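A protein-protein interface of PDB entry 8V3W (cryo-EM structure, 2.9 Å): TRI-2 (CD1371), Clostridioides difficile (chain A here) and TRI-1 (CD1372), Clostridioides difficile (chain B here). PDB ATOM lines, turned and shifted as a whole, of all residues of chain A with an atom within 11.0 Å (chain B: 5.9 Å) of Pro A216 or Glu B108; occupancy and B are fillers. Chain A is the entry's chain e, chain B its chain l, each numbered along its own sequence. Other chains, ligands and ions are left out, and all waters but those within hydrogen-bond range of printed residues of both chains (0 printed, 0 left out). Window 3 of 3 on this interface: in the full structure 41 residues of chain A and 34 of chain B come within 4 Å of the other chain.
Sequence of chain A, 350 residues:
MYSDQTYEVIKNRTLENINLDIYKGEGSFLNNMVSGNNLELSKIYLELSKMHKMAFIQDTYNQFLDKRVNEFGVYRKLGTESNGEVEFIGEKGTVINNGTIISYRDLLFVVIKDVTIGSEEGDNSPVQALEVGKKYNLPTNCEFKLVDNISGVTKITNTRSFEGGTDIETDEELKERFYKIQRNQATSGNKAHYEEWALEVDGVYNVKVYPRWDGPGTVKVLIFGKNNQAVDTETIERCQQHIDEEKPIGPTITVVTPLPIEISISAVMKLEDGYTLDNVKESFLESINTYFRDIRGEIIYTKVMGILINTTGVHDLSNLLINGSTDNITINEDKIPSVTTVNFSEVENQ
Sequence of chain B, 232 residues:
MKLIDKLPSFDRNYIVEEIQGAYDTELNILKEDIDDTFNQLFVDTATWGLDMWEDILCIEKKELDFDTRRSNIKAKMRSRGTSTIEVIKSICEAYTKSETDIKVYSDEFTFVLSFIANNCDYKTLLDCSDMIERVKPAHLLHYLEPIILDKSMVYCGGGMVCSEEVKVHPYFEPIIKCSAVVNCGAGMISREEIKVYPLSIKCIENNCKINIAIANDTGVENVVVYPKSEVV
O of His B139 is in hydrogen-bond range of N of Gly A217 (3.2 Å). NH1 of Arg A212 sits at hydrogen-bond distance from O of His B139, 3.2 Å away.
Among the printed residues, pairs that only touch across the chains: Tyr A194 with His B139 (3.8 Å), Arg A212 with Leu B141 (3.3 Å), Pro A216 with Glu B108 (3.2 Å), Pro A216 with Phe B109 (3.5 Å), Pro A216 with His B139 (3.99 Å), Gly A217 with Phe B109 (3.4 Å), Thr A218 with His B139 (3.999 Å), Val A219 with His B139 (3.7 Å) and Pro A251 with His B139 (3.3 Å).
Of the printed residues of chain B, Arg A212 touches His B139 and Leu B141. Of the printed residues of chain B, Pro A216 touches Glu B108, Phe B109 and His B139. Of the printed residues of chain B, Thr A218 touches His B139 (3.999 Å). Of the printed residues of chain B, Val A219 touches His B139. Lys A220 touches none of the printed residues of chain B. Thr A252 touches none of the printed residues of chain B. No residue of chain A comes within 4 Å of Tyr B105. No residue of chain A comes within 4 Å of Asp B107. Glu B108 touches just one residue of chain A: Pro A216. Printed residues of chain A within 4 Å of Phe B109: Pro A216 (3.5 Å) and Gly A217 (3.4 Å). No residue of chain A comes within 4 Å of Thr B110. Of the printed residues of chain A, His B139 touches Tyr A194 (3.8 Å), Arg A212 (3.2 Å), Pro A216 (3.99 Å), Gly A217 (3.2 Å), Thr A218 (3.999 Å), Val A219 (3.7 Å) and Pro A251 (3.3 Å). The nearest printed residue of chain B that does not touch Pro A216 is Thr B110 (4.7 Å). The nearest printed residue of chain B that does not touch Gly A217 is Glu B108 (5.8 Å).
Of the 8 printed residues of chain B, 4 touch a printed residue of chain A. Hydrophobic or aromatic side chains of chain B within 4 Å of the printed part of chain A: Phe B109, His B139 and Leu B141. Printed residues of chain A that touch a printed residue of chain B: Tyr A194, Arg A212, Pro A216, Gly A217, Thr A218, Val A219 and Pro A251. Hydrophobic or aromatic side chains of chain A that line the printed part of chain B: Tyr A194, Pro A216, Val A219 and Pro A251. Along chain A the printed residues that touch a printed residue of chain B span positions 194 to 251. Among the printed residues, no Asp or Glu carboxylate lies within 4 Å of a Lys or Arg side-chain nitrogen of the other chain.
The backbone carbonyl oxygen (O) of Phe B109 is in hydrogen-bond range of the backbone NH (N) of Leu B141, at 2.9 Å. O of Glu B108 is in hydrogen-bond range of OG1 of Thr B110 (3.0 Å). O of Thr A252 lies within hydrogen-bond range of N of Val A219. The backbone NH of Arg A212 sits at hydrogen-bond distance from the backbone carbonyl oxygen of Thr A218 (2.8 Å). The backbone NH (N) of Asp A214 lies within hydrogen-bond range of the side-chain hydroxyl (OG1) of Thr A218 (2.9 Å). The backbone carbonyl oxygen of Val A219 sits at hydrogen-bond distance from the backbone NH of Thr A254 (3.0 Å).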
ATOM      1  N   TYR A 194       7.019  20.094  14.909  1.00  0.00           N
ATOM      2  CA  TYR A 194       7.393  21.438  14.478  1.00  0.00           C
ATOM      3  C   TYR A 194       7.179  22.446  15.598  1.00  0.00           C
ATOM      4  O   TYR A 194       8.046  23.290  15.862  1.00  0.00           O
ATOM      5  CB  TYR A 194       6.587  21.840  13.241  1.00  0.00           C
ATOM      6  CG  TYR A 194       7.012  21.144  11.969  1.00  0.00           C
ATOM      7  CD1 TYR A 194       8.193  21.486  11.331  1.00  0.00           C
ATOM      8  CD2 TYR A 194       6.235  20.142  11.410  1.00  0.00           C
ATOM      9  CE1 TYR A 194       8.588  20.855  10.169  1.00  0.00           C
ATOM     10  CE2 TYR A 194       6.623  19.504  10.250  1.00  0.00           C
ATOM     11  CZ  TYR A 194       7.798  19.864   9.633  1.00  0.00           C
ATOM     12  OH  TYR A 194       8.183  19.228   8.475  1.00  0.00           O
ATOM     13  N   TYR A 210       1.618  25.893   9.789  1.00  0.00           N
ATOM     14  CA  TYR A 210       0.736  25.836   8.622  1.00  0.00           C
ATOM     15  C   TYR A 210       1.260  24.826   7.610  1.00  0.00           C
ATOM     16  O   TYR A 210       2.170  25.144   6.823  1.00  0.00           O
ATOM     17  CB  TYR A 210       0.606  27.213   7.977  1.00  0.00           C
ATOM     18  CG  TYR A 210      -0.089  28.238   8.837  1.00  0.00           C
ATOM     19  CD1 TYR A 210      -1.475  28.343   8.842  1.00  0.00           C
ATOM     20  CD2 TYR A 210       0.637  29.113   9.634  1.00  0.00           C
ATOM     21  CE1 TYR A 210      -2.119  29.283   9.623  1.00  0.00           C
ATOM     22  CE2 TYR A 210       0.004  30.058  10.418  1.00  0.00           C
ATOM     23  CZ  TYR A 210      -1.375  30.138  10.408  1.00  0.00           C
ATOM     24  OH  TYR A 210      -2.012  31.076  11.188  1.00  0.00           O
ATOM     25  N   PRO A 211       0.726  23.608   7.586  1.00  0.00           N
ATOM     26  CA  PRO A 211       1.195  22.615   6.612  1.00  0.00           C
ATOM     27  C   PRO A 211       0.736  22.943   5.199  1.00  0.00           C
ATOM     28  O   PRO A 211      -0.275  23.619   4.989  1.00  0.00           O
ATOM     29  CB  PRO A 211       0.571  21.302   7.105  1.00  0.00           C
ATOM     30  CG  PRO A 211       0.051  21.596   8.497  1.00  0.00           C
ATOM     31  CD  PRO A 211      -0.277  23.050   8.505  1.00  0.00           C
ATOM     32  N   ARG A 212       1.512  22.449   4.228  1.00  0.00           N
ATOM     33  CA  ARG A 212       1.247  22.555   2.792  1.00  0.00           C
ATOM     34  C   ARG A 212       0.749  23.933   2.368  1.00  0.00           C
ATOM     35  O   ARG A 212      -0.106  24.053   1.484  1.00  0.00           O
ATOM     36  CB  ARG A 212       0.270  21.460   2.342  1.00  0.00           C
ATOM     37  CG  ARG A 212      -1.163  21.573   2.845  1.00  0.00           C
ATOM     38  CD  ARG A 212      -1.881  20.240   2.759  1.00  0.00           C
ATOM     39  NE  ARG A 212      -1.501  19.338   3.839  1.00  0.00           N
ATOM     40  CZ  ARG A 212      -0.546  18.422   3.754  1.00  0.00           C
ATOM     41  NH1 ARG A 212       0.168  18.267   2.652  1.00  0.00           N
ATOM     42  NH2 ARG A 212      -0.303  17.641   4.802  1.00  0.00           N
ATOM     43  N   TRP A 213       1.303  24.982   2.976  1.00  0.00           N
ATOM     44  CA  TRP A 213       0.927  26.340   2.602  1.00  0.00           C
ATOM     45  C   TRP A 213       1.316  26.653   1.162  1.00  0.00           C
ATOM     46  O   TRP A 213       0.629  27.431   0.490  1.00  0.00           O
ATOM     47  CB  TRP A 213       1.581  27.341   3.551  1.00  0.00           C
ATOM     48  CG  TRP A 213       3.047  27.464   3.312  1.00  0.00           C
ATOM     49  CD1 TRP A 213       4.014  26.570   3.666  1.00  0.00           C
ATOM     50  CD2 TRP A 213       3.717  28.539   2.648  1.00  0.00           C
ATOM     51  NE1 TRP A 213       5.247  27.026   3.270  1.00  0.00           N
ATOM     52  CE2 TRP A 213       5.092  28.233   2.641  1.00  0.00           C
ATOM     53  CE3 TRP A 213       3.290  29.733   2.062  1.00  0.00           C
ATOM     54  CZ2 TRP A 213       6.040  29.076   2.070  1.00  0.00           C
ATOM     55  CZ3 TRP A 213       4.232  30.569   1.498  1.00  0.00           C
ATOM     56  CH2 TRP A 213       5.593  30.238   1.507  1.00  0.00           C
ATOM     57  N   ASP A 214       2.409  26.066   0.675  1.00  0.00           N
ATOM     58  CA  ASP A 214       2.882  26.333  -0.677  1.00  0.00           C
ATOM     59  C   ASP A 214       2.934  24.951  -1.334  1.00  0.00           C
ATOM     60  O   ASP A 214       3.986  24.479  -1.775  1.00  0.00           O
ATOM     61  CB  ASP A 214       4.229  27.091  -0.619  1.00  0.00           C
ATOM     62  CG  ASP A 214       5.074  27.003  -1.904  1.00  0.00           C
ATOM     63  OD1 ASP A 214       4.592  26.560  -2.965  1.00  0.00           O
ATOM     64  OD2 ASP A 214       6.208  27.525  -1.879  1.00  0.00           O
ATOM     65  N   GLY A 215       1.815  24.239  -1.294  1.00  0.00           N
ATOM     66  CA  GLY A 215       1.752  22.916  -1.863  1.00  0.00           C
ATOM     67  C   GLY A 215       2.449  21.893  -0.990  1.00  0.00           C
ATOM     68  O   GLY A 215       2.912  22.196   0.113  1.00  0.00           O
ATOM     69  N   PRO A 216       2.549  20.659  -1.479  1.00  0.00           N
ATOM     70  CA  PRO A 216       3.171  19.596  -0.682  1.00  0.00           C
ATOM     71  C   PRO A 216       4.645  19.873  -0.424  1.00  0.00           C
ATOM     72  O   PRO A 216       5.335  20.500  -1.231  1.00  0.00           O
ATOM     73  CB  PRO A 216       2.981  18.344  -1.550  1.00  0.00           C
ATOM     74  CG  PRO A 216       1.920  18.719  -2.557  1.00  0.00           C
ATOM     75  CD  PRO A 216       2.128  20.175  -2.804  1.00  0.00           C
ATOM     76  N   GLY A 217       5.123  19.399   0.724  1.00  0.00           N
ATOM     77  CA  GLY A 217       6.512  19.583   1.089  1.00  0.00           C
ATOM     78  C   GLY A 217       6.880  20.973   1.544  1.00  0.00           C
ATOM     79  O   GLY A 217       8.062  21.326   1.528  1.00  0.00           O
ATOM     80  N   THR A 218       5.903  21.780   1.942  1.00  0.00           N
ATOM     81  CA  THR A 218       6.146  23.126   2.439  1.00  0.00           C
ATOM     82  C   THR A 218       5.439  23.298   3.774  1.00  0.00           C
ATOM     83  O   THR A 218       4.250  22.989   3.896  1.00  0.00           O
ATOM     84  CB  THR A 218       5.657  24.180   1.442  1.00  0.00           C
ATOM     85  OG1 THR A 218       4.283  23.927   1.122  1.00  0.00           O
ATOM     86  CG2 THR A 218       6.488  24.139   0.177  1.00  0.00           C
ATOM     87  N   VAL A 219       6.171  23.792   4.770  1.00  0.00           N
ATOM     88  CA  VAL A 219       5.631  24.048   6.098  1.00  0.00           C
ATOM     89  C   VAL A 219       5.842  25.518   6.423  1.00  0.00           C
ATOM     90  O   VAL A 219       6.968  26.021   6.344  1.00  0.00           O
ATOM     91  CB  VAL A 219       6.287  23.150   7.163  1.00  0.00           C
ATOM     92  CG1 VAL A 219       5.807  23.538   8.551  1.00  0.00           C
ATOM     93  CG2 VAL A 219       5.985  21.689   6.881  1.00  0.00           C
ATOM     94  N   LYS A 220       4.762  26.200   6.789  1.00  0.00           N
ATOM     95  CA  LYS A 220       4.811  27.609   7.160  1.00  0.00           C
ATOM     96  C   LYS A 220       4.800  27.709   8.678  1.00  0.00           C
ATOM     97  O   LYS A 220       3.843  27.274   9.327  1.00  0.00           O
ATOM     98  CB  LYS A 220       3.633  28.374   6.556  1.00  0.00           C
ATOM     99  CG  LYS A 220       3.802  29.884   6.541  1.00  0.00           C
ATOM    100  CD  LYS A 220       2.671  30.550   5.774  1.00  0.00           C
ATOM    101  CE  LYS A 220       2.822  32.063   5.765  1.00  0.00           C
ATOM    102  NZ  LYS A 220       1.683  32.734   5.083  1.00  0.00           N
ATOM    103  N   GLY A 250      14.198  16.742   3.172  1.00  0.00           N
ATOM    104  CA  GLY A 250      13.296  16.887   2.051  1.00  0.00           C
ATOM    105  C   GLY A 250      12.315  18.044   2.155  1.00  0.00           C
ATOM    106  O   GLY A 250      12.094  18.770   1.180  1.00  0.00           O
ATOM    107  N   PRO A 251      11.703  18.243   3.323  1.00  0.00           N
ATOM    108  CA  PRO A 251      10.827  19.406   3.501  1.00  0.00           C
ATOM    109  C   PRO A 251      11.588  20.721   3.439  1.00  0.00           C
ATOM    110  O   PRO A 251      12.804  20.785   3.625  1.00  0.00           O
ATOM    111  CB  PRO A 251      10.230  19.192   4.896  1.00  0.00           C
ATOM    112  CG  PRO A 251      10.258  17.738   5.090  1.00  0.00           C
ATOM    113  CD  PRO A 251      11.441  17.210   4.341  1.00  0.00           C
ATOM    114  N   THR A 252      10.837  21.787   3.164  1.00  0.00           N
ATOM    115  CA  THR A 252      11.352  23.149   3.160  1.00  0.00           C
ATOM    116  C   THR A 252      10.527  23.989   4.125  1.00  0.00           C
ATOM    117  O   THR A 252       9.293  23.959   4.079  1.00  0.00           O
ATOM    118  CB  THR A 252      11.309  23.756   1.756  1.00  0.00           C
ATOM    119  OG1 THR A 252      12.024  22.912   0.848  1.00  0.00           O
ATOM    120  CG2 THR A 252      11.941  25.138   1.755  1.00  0.00           C
ATOM    121  N   ILE A 253      11.207  24.743   4.986  1.00  0.00           N
ATOM    122  CA  ILE A 253      10.570  25.485   6.069  1.00  0.00           C
ATOM    123  C   ILE A 253      10.632  26.973   5.763  1.00  0.00           C
ATOM    124  O   ILE A 253      11.705  27.510   5.463  1.00  0.00           O
ATOM    125  CB  ILE A 253      11.232  25.180   7.423  1.00  0.00           C
ATOM    126  CG1 ILE A 253      11.277  23.672   7.667  1.00  0.00           C
ATOM    127  CG2 ILE A 253      10.494  25.889   8.543  1.00  0.00           C
ATOM    128  CD1 ILE A 253       9.929  23.000   7.582  1.00  0.00           C
ATOM    129  N   THR A 254       9.483  27.638   5.849  1.00  0.00           N
ATOM    130  CA  THR A 254       9.379  29.079   5.669  1.00  0.00           C
ATOM    131  C   THR A 254       8.786  29.693   6.929  1.00  0.00           C
ATOM    132  O   THR A 254       7.791  29.189   7.461  1.00  0.00           O
ATOM    133  CB  THR A 254       8.517  29.427   4.454  1.00  0.00           C
ATOM    134  OG1 THR A 254       8.926  28.634   3.334  1.00  0.00           O
ATOM    135  CG2 THR A 254       8.661  30.900   4.106  1.00  0.00           C
ATOM    136  N   TYR B 105       4.374   8.645  -2.555  1.00  0.00           N
ATOM    137  CA  TYR B 105       4.784   9.342  -3.772  1.00  0.00           C
ATOM    138  C   TYR B 105       5.731  10.465  -3.360  1.00  0.00           C
ATOM    139  O   TYR B 105       5.289  11.554  -2.982  1.00  0.00           O
ATOM    140  CB  TYR B 105       3.568   9.864  -4.529  1.00  0.00           C
ATOM    141  CG  TYR B 105       2.535   8.795  -4.802  1.00  0.00           C
ATOM    142  CD1 TYR B 105       2.651   7.951  -5.898  1.00  0.00           C
ATOM    143  CD2 TYR B 105       1.448   8.622  -3.955  1.00  0.00           C
ATOM    144  CE1 TYR B 105       1.711   6.970  -6.146  1.00  0.00           C
ATOM    145  CE2 TYR B 105       0.503   7.644  -4.196  1.00  0.00           C
ATOM    146  CZ  TYR B 105       0.639   6.822  -5.292  1.00  0.00           C
ATOM    147  OH  TYR B 105      -0.300   5.847  -5.531  1.00  0.00           O
ATOM    148  N   SER B 106       7.035  10.189  -3.435  1.00  0.00           N
ATOM    149  CA  SER B 106       8.032  11.141  -2.955  1.00  0.00           C
ATOM    150  C   SER B 106       8.004  12.437  -3.753  1.00  0.00           C
ATOM    151  O   SER B 106       8.152  13.525  -3.186  1.00  0.00           O
ATOM    152  CB  SER B 106       9.423  10.511  -3.010  1.00  0.00           C
ATOM    153  OG  SER B 106       9.370   9.133  -2.684  1.00  0.00           O
ATOM    154  N   ASP B 107       7.834  12.342  -5.073  1.00  0.00           N
ATOM    155  CA  ASP B 107       7.807  13.543  -5.901  1.00  0.00           C
ATOM    156  C   ASP B 107       6.604  14.417  -5.569  1.00  0.00           C
ATOM    157  O   ASP B 107       6.715  15.648  -5.526  1.00  0.00           O
ATOM    158  CB  ASP B 107       7.800  13.159  -7.379  1.00  0.00           C
ATOM    159  CG  ASP B 107       8.913  12.197  -7.734  1.00  0.00           C
ATOM    160  OD1 ASP B 107       9.928  12.164  -7.007  1.00  0.00           O
ATOM    161  OD2 ASP B 107       8.773  11.469  -8.739  1.00  0.00           O
ATOM    162  N   GLU B 108       5.446  13.800  -5.341  1.00  0.00           N
ATOM    163  CA  GLU B 108       4.236  14.527  -4.981  1.00  0.00           C
ATOM    164  C   GLU B 108       4.122  14.795  -3.487  1.00  0.00           C
ATOM    165  O   GLU B 108       3.214  15.527  -3.076  1.00  0.00           O
ATOM    166  CB  GLU B 108       2.995  13.759  -5.454  1.00  0.00           C
ATOM    167  CG  GLU B 108       3.012  13.352  -6.926  1.00  0.00           C
ATOM    168  CD  GLU B 108       3.738  12.043  -7.182  1.00  0.00           C
ATOM    169  OE1 GLU B 108       4.840  11.849  -6.629  1.00  0.00           O
ATOM    170  OE2 GLU B 108       3.201  11.203  -7.933  1.00  0.00           O
ATOM    171  N   PHE B 109       5.017  14.231  -2.675  1.00  0.00           N
ATOM    172  CA  PHE B 109       4.981  14.386  -1.219  1.00  0.00           C
ATOM    173  C   PHE B 109       3.615  13.995  -0.661  1.00  0.00           C
ATOM    174  O   PHE B 109       3.048  14.678   0.194  1.00  0.00           O
ATOM    175  CB  PHE B 109       5.349  15.812  -0.786  1.00  0.00           C
ATOM    176  CG  PHE B 109       6.739  16.243  -1.177  1.00  0.00           C
ATOM    177  CD1 PHE B 109       7.141  16.264  -2.502  1.00  0.00           C
ATOM    178  CD2 PHE B 109       7.625  16.692  -0.214  1.00  0.00           C
ATOM    179  CE1 PHE B 109       8.413  16.674  -2.851  1.00  0.00           C
ATOM    180  CE2 PHE B 109       8.896  17.105  -0.556  1.00  0.00           C
ATOM    181  CZ  PHE B 109       9.289  17.098  -1.875  1.00  0.00           C
ATOM    182  N   THR B 110       3.077  12.883  -1.156  1.00  0.00           N
ATOM    183  CA  THR B 110       1.742  12.440  -0.788  1.00  0.00           C
ATOM    184  C   THR B 110       1.735  10.933  -0.586  1.00  0.00           C
ATOM    185  O   THR B 110       2.305  10.191  -1.390  1.00  0.00           O
ATOM    186  CB  THR B 110       0.711  12.828  -1.858  1.00  0.00           C
ATOM    187  OG1 THR B 110       0.748  14.246  -2.065  1.00  0.00           O
ATOM    188  CG2 THR B 110      -0.691  12.406  -1.442  1.00  0.00           C
ATOM    189  N   HIS B 139       4.324  18.353   6.321  1.00  0.00           N
ATOM    190  CA  HIS B 139       4.518  18.678   4.912  1.00  0.00           C
ATOM    191  C   HIS B 139       3.867  17.640   4.006  1.00  0.00           C
ATOM    192  O   HIS B 139       3.300  17.983   2.962  1.00  0.00           O
ATOM    193  CB  HIS B 139       6.010  18.800   4.606  1.00  0.00           C
ATOM    194  CG  HIS B 139       6.745  17.495   4.650  1.00  0.00           C
ATOM    195  ND1 HIS B 139       6.903  16.769   5.811  1.00  0.00           N
ATOM    196  CD2 HIS B 139       7.352  16.781   3.673  1.00  0.00           C
ATOM    197  CE1 HIS B 139       7.582  15.668   5.548  1.00  0.00           C
ATOM    198  NE2 HIS B 139       7.867  15.650   4.259  1.00  0.00           N
ATOM    199  N   LEU B 141       1.253  14.943   2.454  1.00  0.00           N
ATOM    200  CA  LEU B 141      -0.186  14.981   2.242  1.00  0.00           C
ATOM    201  C   LEU B 141      -0.761  13.575   2.350  1.00  0.00           C
ATOM    202  O   LEU B 141      -0.166  12.610   1.860  1.00  0.00           O
ATOM    203  CB  LEU B 141      -0.522  15.584   0.875  1.00  0.00           C
ATOM    204  CG  LEU B 141      -1.985  15.516   0.423  1.00  0.00           C
ATOM    205  CD1 LEU B 141      -2.839  16.497   1.203  1.00  0.00           C
ATOM    206  CD2 LEU B 141      -2.094  15.774  -1.071  1.00  0.00           C
